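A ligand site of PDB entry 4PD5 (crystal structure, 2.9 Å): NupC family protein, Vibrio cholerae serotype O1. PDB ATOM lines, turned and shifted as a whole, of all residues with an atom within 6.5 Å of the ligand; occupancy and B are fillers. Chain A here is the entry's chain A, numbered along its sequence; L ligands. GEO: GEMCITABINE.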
ATOM      1  N   VAL A 158      -0.615 -10.148 -26.039  1.00  0.00           N
ATOM      2  CA  VAL A 158      -0.872  -8.717 -25.941  1.00  0.00           C
ATOM      3  C   VAL A 158      -2.358  -8.374 -26.040  1.00  0.00           C
ATOM      4  O   VAL A 158      -3.179  -9.232 -26.374  1.00  0.00           O
ATOM      5  CB  VAL A 158      -0.107  -7.939 -27.037  1.00  0.00           C
ATOM      6  CG1 VAL A 158       1.391  -8.132 -26.879  1.00  0.00           C
ATOM      7  CG2 VAL A 158      -0.569  -8.377 -28.415  1.00  0.00           C
ATOM      8  N   GLY A 159      -2.681  -7.118 -25.765  1.00  0.00           N
ATOM      9  CA  GLY A 159      -4.060  -6.663 -25.702  1.00  0.00           C
ATOM     10  C   GLY A 159      -4.755  -6.495 -27.029  1.00  0.00           C
ATOM     11  O   GLY A 159      -4.159  -6.682 -28.093  1.00  0.00           O
ATOM     12  N   GLN A 160      -6.026  -6.119 -26.970  1.00  0.00           N
ATOM     13  CA  GLN A 160      -6.891  -6.025 -28.139  1.00  0.00           C
ATOM     14  C   GLN A 160      -6.477  -4.927 -29.110  1.00  0.00           C
ATOM     15  O   GLN A 160      -6.752  -5.006 -30.313  1.00  0.00           O
ATOM     16  CB  GLN A 160      -8.341  -5.814 -27.709  1.00  0.00           C
ATOM     17  CG  GLN A 160      -8.529  -4.684 -26.720  1.00  0.00           C
ATOM     18  CD  GLN A 160      -9.961  -4.588 -26.219  1.00  0.00           C
ATOM     19  OE1 GLN A 160     -10.887  -5.095 -26.863  1.00  0.00           O
ATOM     20  NE2 GLN A 160     -10.148  -3.948 -25.071  1.00  0.00           N
ATOM     21  N   THR A 161      -5.837  -3.882 -28.598  1.00  0.00           N
ATOM     22  CA  THR A 161      -5.453  -2.746 -29.430  1.00  0.00           C
ATOM     23  C   THR A 161      -3.996  -2.831 -29.875  1.00  0.00           C
ATOM     24  O   THR A 161      -3.560  -2.067 -30.746  1.00  0.00           O
ATOM     25  CB  THR A 161      -5.665  -1.410 -28.680  1.00  0.00           C
ATOM     26  OG1 THR A 161      -4.896  -1.407 -27.468  1.00  0.00           O
ATOM     27  CG2 THR A 161      -7.123  -1.215 -28.342  1.00  0.00           C
ATOM     28  N   GLU A 162      -3.253  -3.771 -29.295  1.00  0.00           N
ATOM     29  CA  GLU A 162      -1.837  -3.938 -29.627  1.00  0.00           C
ATOM     30  C   GLU A 162      -1.612  -5.102 -30.581  1.00  0.00           C
ATOM     31  O   GLU A 162      -0.648  -5.115 -31.341  1.00  0.00           O
ATOM     32  CB  GLU A 162      -1.011  -4.155 -28.350  1.00  0.00           C
ATOM     33  CG  GLU A 162      -0.867  -2.919 -27.472  1.00  0.00           C
ATOM     34  CD  GLU A 162      -2.116  -2.625 -26.666  1.00  0.00           C
ATOM     35  OE1 GLU A 162      -3.017  -3.497 -26.613  1.00  0.00           O
ATOM     36  OE2 GLU A 162      -2.190  -1.530 -26.077  1.00  0.00           O
ATOM     37  N   GLY A 186      -9.296  -9.969 -29.752  1.00  0.00           N
ATOM     38  CA  GLY A 186      -8.922  -9.169 -28.606  1.00  0.00           C
ATOM     39  C   GLY A 186      -9.961  -9.181 -27.508  1.00  0.00           C
ATOM     40  O   GLY A 186      -9.638  -8.992 -26.332  1.00  0.00           O
ATOM     41  N   SER A 189      -9.643 -12.598 -25.560  1.00  0.00           N
ATOM     42  CA  SER A 189      -8.399 -12.796 -24.824  1.00  0.00           C
ATOM     43  C   SER A 189      -8.100 -11.643 -23.883  1.00  0.00           C
ATOM     44  O   SER A 189      -8.889 -10.717 -23.732  1.00  0.00           O
ATOM     45  CB  SER A 189      -7.239 -12.988 -25.805  1.00  0.00           C
ATOM     46  OG  SER A 189      -7.139 -11.880 -26.685  1.00  0.00           O
ATOM     47  N   ILE A 190      -6.937 -11.720 -23.238  1.00  0.00           N
ATOM     48  CA  ILE A 190      -6.446 -10.652 -22.380  1.00  0.00           C
ATOM     49  C   ILE A 190      -5.071 -10.206 -22.837  1.00  0.00           C
ATOM     50  O   ILE A 190      -4.722 -10.350 -24.012  1.00  0.00           O
ATOM     51  CB  ILE A 190      -6.387 -11.091 -20.901  1.00  0.00           C
ATOM     52  CG1 ILE A 190      -5.525 -12.354 -20.753  1.00  0.00           C
ATOM     53  CG2 ILE A 190      -7.782 -11.353 -20.367  1.00  0.00           C
ATOM     54  CD1 ILE A 190      -5.272 -12.744 -19.314  1.00  0.00           C
ATOM     55  N   ALA A 191      -4.284  -9.654 -21.926  1.00  0.00           N
ATOM     56  CA  ALA A 191      -2.918  -9.253 -22.225  1.00  0.00           C
ATOM     57  C   ALA A 191      -1.952  -9.852 -21.211  1.00  0.00           C
ATOM     58  O   ALA A 191      -2.350 -10.232 -20.112  1.00  0.00           O
ATOM     59  CB  ALA A 191      -2.792  -7.746 -22.259  1.00  0.00           C
ATOM     60  N   VAL A 194      -1.863  -7.750 -17.674  1.00  0.00           N
ATOM     61  CA  VAL A 194      -2.947  -7.981 -16.735  1.00  0.00           C
ATOM     62  C   VAL A 194      -3.006  -9.433 -16.274  1.00  0.00           C
ATOM     63  O   VAL A 194      -3.493  -9.738 -15.187  1.00  0.00           O
ATOM     64  CB  VAL A 194      -4.316  -7.597 -17.334  1.00  0.00           C
ATOM     65  CG1 VAL A 194      -4.415  -6.082 -17.496  1.00  0.00           C
ATOM     66  CG2 VAL A 194      -4.536  -8.301 -18.669  1.00  0.00           C
ATOM     67  N   TYR A 198      -3.489 -10.546 -12.511  1.00  0.00           N
ATOM     68  CA  TYR A 198      -4.498 -11.458 -11.959  1.00  0.00           C
ATOM     69  C   TYR A 198      -3.839 -12.591 -11.185  1.00  0.00           C
ATOM     70  O   TYR A 198      -4.358 -13.061 -10.171  1.00  0.00           O
ATOM     71  CB  TYR A 198      -5.385 -12.020 -13.066  1.00  0.00           C
ATOM     72  CG  TYR A 198      -6.101 -10.957 -13.861  1.00  0.00           C
ATOM     73  CD1 TYR A 198      -6.562  -9.804 -13.249  1.00  0.00           C
ATOM     74  CD2 TYR A 198      -6.316 -11.103 -15.230  1.00  0.00           C
ATOM     75  CE1 TYR A 198      -7.221  -8.825 -13.966  1.00  0.00           C
ATOM     76  CE2 TYR A 198      -6.967 -10.119 -15.957  1.00  0.00           C
ATOM     77  CZ  TYR A 198      -7.414  -8.986 -15.323  1.00  0.00           C
ATOM     78  OH  TYR A 198      -8.072  -8.011 -16.031  1.00  0.00           O
ATOM     79  N   LEU A 265      -1.374   2.588 -18.355  1.00  0.00           N
ATOM     80  CA  LEU A 265      -2.364   1.533 -18.158  1.00  0.00           C
ATOM     81  C   LEU A 265      -2.616   1.293 -16.674  1.00  0.00           C
ATOM     82  O   LEU A 265      -3.759   1.124 -16.256  1.00  0.00           O
ATOM     83  CB  LEU A 265      -1.897   0.236 -18.840  1.00  0.00           C
ATOM     84  CG  LEU A 265      -2.804  -0.989 -18.669  1.00  0.00           C
ATOM     85  CD1 LEU A 265      -4.163  -0.765 -19.324  1.00  0.00           C
ATOM     86  CD2 LEU A 265      -2.130  -2.230 -19.248  1.00  0.00           C
ATOM     87  N   VAL A 269      -6.236   1.618 -14.837  1.00  0.00           N
ATOM     88  CA  VAL A 269      -6.847   0.495 -14.143  1.00  0.00           C
ATOM     89  C   VAL A 269      -7.127   0.850 -12.684  1.00  0.00           C
ATOM     90  O   VAL A 269      -8.206   0.552 -12.154  1.00  0.00           O
ATOM     91  CB  VAL A 269      -5.956  -0.760 -14.192  1.00  0.00           C
ATOM     92  CG1 VAL A 269      -6.488  -1.851 -13.278  1.00  0.00           C
ATOM     93  CG2 VAL A 269      -5.841  -1.274 -15.627  1.00  0.00           C
ATOM     94  N   MET A 272     -10.017   3.285 -12.331  1.00  0.00           N
ATOM     95  CA  MET A 272     -11.247   2.582 -12.675  1.00  0.00           C
ATOM     96  C   MET A 272     -11.745   1.733 -11.504  1.00  0.00           C
ATOM     97  O   MET A 272     -12.934   1.710 -11.206  1.00  0.00           O
ATOM     98  CB  MET A 272     -11.039   1.722 -13.916  1.00  0.00           C
ATOM     99  CG  MET A 272     -12.214   0.829 -14.291  1.00  0.00           C
ATOM    100  SD  MET A 272     -12.153  -0.796 -13.504  1.00  0.00           S
ATOM    101  CE  MET A 272     -10.548  -1.374 -14.051  1.00  0.00           C
ATOM    102  N   ALA A 336     -19.326  -4.932 -16.326  1.00  0.00           N
ATOM    103  CA  ALA A 336     -18.234  -4.014 -16.049  1.00  0.00           C
ATOM    104  C   ALA A 336     -16.991  -4.436 -16.831  1.00  0.00           C
ATOM    105  O   ALA A 336     -16.868  -4.131 -18.020  1.00  0.00           O
ATOM    106  CB  ALA A 336     -17.925  -3.980 -14.554  1.00  0.00           C
ATOM    107  N   ASN A 337     -16.071  -5.122 -16.162  1.00  0.00           N
ATOM    108  CA  ASN A 337     -14.911  -5.711 -16.815  1.00  0.00           C
ATOM    109  C   ASN A 337     -14.354  -6.849 -15.964  1.00  0.00           C
ATOM    110  O   ASN A 337     -14.755  -7.033 -14.817  1.00  0.00           O
ATOM    111  CB  ASN A 337     -13.837  -4.653 -17.088  1.00  0.00           C
ATOM    112  CG  ASN A 337     -13.384  -3.936 -15.835  1.00  0.00           C
ATOM    113  OD1 ASN A 337     -12.563  -4.445 -15.079  1.00  0.00           O
ATOM    114  ND2 ASN A 337     -13.928  -2.746 -15.610  1.00  0.00           N
ATOM    115  N   GLU A 338     -13.422  -7.596 -16.529  1.00  0.00           N
ATOM    116  CA  GLU A 338     -12.918  -8.806 -15.875  1.00  0.00           C
ATOM    117  C   GLU A 338     -12.012  -8.481 -14.692  1.00  0.00           C
ATOM    118  O   GLU A 338     -11.823  -9.316 -13.807  1.00  0.00           O
ATOM    119  CB  GLU A 338     -12.170  -9.682 -16.882  1.00  0.00           C
ATOM    120  CG  GLU A 338     -10.718  -9.286 -17.130  1.00  0.00           C
ATOM    121  CD  GLU A 338     -10.573  -7.975 -17.867  1.00  0.00           C
ATOM    122  OE1 GLU A 338     -11.568  -7.504 -18.472  1.00  0.00           O
ATOM    123  OE2 GLU A 338      -9.465  -7.402 -17.853  1.00  0.00           O
ATOM    124  N   PHE A 339     -11.457  -7.279 -14.670  1.00  0.00           N
ATOM    125  CA  PHE A 339     -10.567  -6.872 -13.583  1.00  0.00           C
ATOM    126  C   PHE A 339     -11.375  -6.677 -12.301  1.00  0.00           C
ATOM    127  O   PHE A 339     -10.953  -7.102 -11.226  1.00  0.00           O
ATOM    128  CB  PHE A 339      -9.817  -5.586 -13.946  1.00  0.00           C
ATOM    129  CG  PHE A 339      -8.415  -5.538 -13.415  1.00  0.00           C
ATOM    130  CD1 PHE A 339      -7.339  -5.457 -14.284  1.00  0.00           C
ATOM    131  CD2 PHE A 339      -8.171  -5.592 -12.055  1.00  0.00           C
ATOM    132  CE1 PHE A 339      -6.042  -5.418 -13.796  1.00  0.00           C
ATOM    133  CE2 PHE A 339      -6.884  -5.546 -11.562  1.00  0.00           C
ATOM    134  CZ  PHE A 339      -5.820  -5.461 -12.439  1.00  0.00           C
ATOM    135  N   VAL A 340     -12.529  -6.032 -12.432  1.00  0.00           N
ATOM    136  CA  VAL A 340     -13.423  -5.825 -11.296  1.00  0.00           C
ATOM    137  C   VAL A 340     -13.985  -7.160 -10.816  1.00  0.00           C
ATOM    138  O   VAL A 340     -14.135  -7.396  -9.617  1.00  0.00           O
ATOM    139  CB  VAL A 340     -14.588  -4.881 -11.652  1.00  0.00           C
ATOM    140  CG1 VAL A 340     -15.458  -4.621 -10.433  1.00  0.00           C
ATOM    141  CG2 VAL A 340     -14.051  -3.572 -12.205  1.00  0.00           C
ATOM    142  N   GLY A 371     -11.013 -12.678 -20.119  1.00  0.00           N
ATOM    143  CA  GLY A 371     -11.314 -12.043 -21.397  1.00  0.00           C
ATOM    144  C   GLY A 371     -11.660 -10.572 -21.248  1.00  0.00           C
ATOM    145  O   GLY A 371     -12.202 -10.147 -20.226  1.00  0.00           O
ATOM    146  N   PHE A 372     -11.353  -9.791 -22.279  1.00  0.00           N
ATOM    147  CA  PHE A 372     -11.650  -8.362 -22.286  1.00  0.00           C
ATOM    148  C   PHE A 372     -13.045  -8.086 -22.838  1.00  0.00           C
ATOM    149  O   PHE A 372     -13.370  -6.954 -23.202  1.00  0.00           O
ATOM    150  CB  PHE A 372     -10.615  -7.596 -23.109  1.00  0.00           C
ATOM    151  CG  PHE A 372      -9.265  -7.496 -22.450  1.00  0.00           C
ATOM    152  CD1 PHE A 372      -9.099  -7.835 -21.120  1.00  0.00           C
ATOM    153  CD2 PHE A 372      -8.169  -7.042 -23.170  1.00  0.00           C
ATOM    154  CE1 PHE A 372      -7.856  -7.736 -20.523  1.00  0.00           C
ATOM    155  CE2 PHE A 372      -6.927  -6.943 -22.573  1.00  0.00           C
ATOM    156  CZ  PHE A 372      -6.771  -7.288 -21.254  1.00  0.00           C
ATOM    157  N   ALA A 373     -13.872  -9.120 -22.906  1.00  0.00           N
ATOM    158  CA  ALA A 373     -15.213  -9.016 -23.482  1.00  0.00           C
ATOM    159  C   ALA A 373     -16.173  -8.250 -22.577  1.00  0.00           C
ATOM    160  O   ALA A 373     -16.732  -8.810 -21.639  1.00  0.00           O
ATOM    161  CB  ALA A 373     -15.760 -10.390 -23.793  1.00  0.00           C
ATOM    162  N   ASN A 374     -16.355  -6.964 -22.876  1.00  0.00           N
ATOM    163  CA  ASN A 374     -17.351  -6.153 -22.188  1.00  0.00           C
ATOM    164  C   ASN A 374     -17.783  -4.977 -23.063  1.00  0.00           C
ATOM    165  O   ASN A 374     -17.136  -4.659 -24.058  1.00  0.00           O
ATOM    166  CB  ASN A 374     -16.809  -5.642 -20.846  1.00  0.00           C
ATOM    167  CG  ASN A 374     -15.514  -4.863 -20.991  1.00  0.00           C
ATOM    168  OD1 ASN A 374     -15.529  -3.680 -21.334  1.00  0.00           O
ATOM    169  ND2 ASN A 374     -14.396  -5.529 -20.734  1.00  0.00           N
ATOM    170  N   SER A 376     -17.725  -1.851 -22.567  1.00  0.00           N
ATOM    171  CA  SER A 376     -16.819  -0.712 -22.533  1.00  0.00           C
ATOM    172  C   SER A 376     -15.649  -0.879 -23.495  1.00  0.00           C
ATOM    173  O   SER A 376     -14.945   0.085 -23.821  1.00  0.00           O
ATOM    174  CB  SER A 376     -16.284  -0.480 -21.119  1.00  0.00           C
ATOM    175  OG  SER A 376     -17.345  -0.158 -20.229  1.00  0.00           O
ATOM    176  N   SER A 377     -15.439  -2.106 -23.960  1.00  0.00           N
ATOM    177  CA  SER A 377     -14.330  -2.411 -24.861  1.00  0.00           C
ATOM    178  C   SER A 377     -14.647  -1.982 -26.297  1.00  0.00           C
ATOM    179  O   SER A 377     -13.749  -1.921 -27.138  1.00  0.00           O
ATOM    180  CB  SER A 377     -13.993  -3.900 -24.808  1.00  0.00           C
ATOM    181  OG  SER A 377     -13.496  -4.264 -23.534  1.00  0.00           O
ATOM    182  N   ILE A 380     -13.136   1.187 -26.662  1.00  0.00           N
ATOM    183  CA  ILE A 380     -11.701   0.944 -26.679  1.00  0.00           C
ATOM    184  C   ILE A 380     -11.253   0.481 -28.063  1.00  0.00           C
ATOM    185  O   ILE A 380     -10.212   0.904 -28.559  1.00  0.00           O
ATOM    186  CB  ILE A 380     -11.294  -0.101 -25.627  1.00  0.00           C
ATOM    187  CG1 ILE A 380     -11.566   0.445 -24.211  1.00  0.00           C
ATOM    188  CG2 ILE A 380      -9.830  -0.476 -25.767  1.00  0.00           C
ATOM    189  CD1 ILE A 380     -11.134  -0.490 -23.107  1.00  0.00           C
HETATM  190  O5' GEO L   1      -8.296  -4.961 -17.683  1.00  0.00           O
HETATM  191  C5' GEO L   1      -9.507  -4.221 -17.397  1.00  0.00           C
HETATM  192  C4' GEO L   1     -10.001  -3.589 -18.693  1.00  0.00           C
HETATM  193  O4' GEO L   1      -8.990  -2.685 -19.227  1.00  0.00           O
HETATM  194  C1' GEO L   1      -8.983  -2.777 -20.649  1.00  0.00           C
HETATM  195  N1  GEO L   1      -7.660  -3.193 -21.124  1.00  0.00           N
HETATM  196  C6  GEO L   1      -6.761  -3.749 -20.246  1.00  0.00           C
HETATM  197  C5  GEO L   1      -5.548  -4.115 -20.674  1.00  0.00           C
HETATM  198  C4  GEO L   1      -5.189  -3.938 -22.046  1.00  0.00           C
HETATM  199  N3  GEO L   1      -6.063  -3.394 -22.889  1.00  0.00           N
HETATM  200  C2  GEO L   1      -7.288  -3.007 -22.461  1.00  0.00           C
HETATM  201  O2  GEO L   1      -8.091  -2.512 -23.258  1.00  0.00           O
HETATM  202  N4  GEO L   1      -3.986  -4.305 -22.473  1.00  0.00           N
HETATM  203  C2' GEO L   1     -10.065  -3.798 -21.013  1.00  0.00           C
HETATM  204  F1  GEO L   1      -9.693  -4.571 -22.056  1.00  0.00           F
HETATM  205  F2  GEO L   1     -11.222  -3.169 -21.291  1.00  0.00           F
HETATM  206  C3' GEO L   1     -10.212  -4.633 -19.754  1.00  0.00           C
HETATM  207  O3' GEO L   1     -11.514  -5.183 -19.666  1.00  0.00           O
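ND2 of Asn 337 sits at hydrogen-bond distance from SD of Met 272, 3.4 Å away.
OD1 of Asn 337 sits at hydrogen-bond distance from N of Phe 339.
The side-chain hydroxyl (OG) of Ser 377 sits at hydrogen-bond distance from the backbone carbonyl oxygen (O) of Phe 372, 2.7 Å away.
ND2 of Asn 374 lies within hydrogen-bond range of O of Phe 372, 3.0 Å away.
The side-chain amide oxygen (OD1) of Asn 337 is in hydrogen-bond range of the backbone NH (N) of Val 340.
The side-chain amide oxygen (OD1) of Asn 374 lies within hydrogen-bond range of the side-chain hydroxyl (OG) of Ser 377.
The backbone carbonyl oxygen (O) of Ser 189 lies within hydrogen-bond range of the backbone NH (N) of Phe 372.
OD1 of Asn 374 sits at hydrogen-bond distance from N of Ser 376 (3.1 Å).
OG of Ser 377 sits close to F2 of the ligand (3.4 Å).
Gly 159 touches the ligand (CA to N4, 3.999 Å).
Ala 191 touches the ligand.
Val 194 touches the ligand (CG1 to C5, 3.9 Å).
CD1 of Leu 265 touches C5 of the ligand (3.9 Å).
CB of Asn 337 touches O3' of the ligand, at 3.5 Å.
Phe 339 touches the ligand.
CG of Phe 372 touches F1 of the ligand, 3.0 Å away.
Ile 380 touches the ligand.
Hydrophobic or aromatic side chains within 4 Å of the ligand: Ala 191, Val 194, Leu 265, Phe 339, Phe 372 and Ile 380.
Of the 26 residues printed, 13 come within 4 Å of the ligand.
The nearest printed residue that does not touch the ligand is Glu 162 (4.3 Å).
OE1 of Glu 338 sits at hydrogen-bond distance from O3' of the ligand (2.6 Å).
ND2 of Asn 374 is in hydrogen-bond range of O3' of the ligand.
O2 of the ligand sits at hydrogen-bond distance from NE2 of Gln 160 (3.1 Å).
OH of Tyr 198 lies within hydrogen-bond range of O5' of the ligand, 3.5 Å away.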
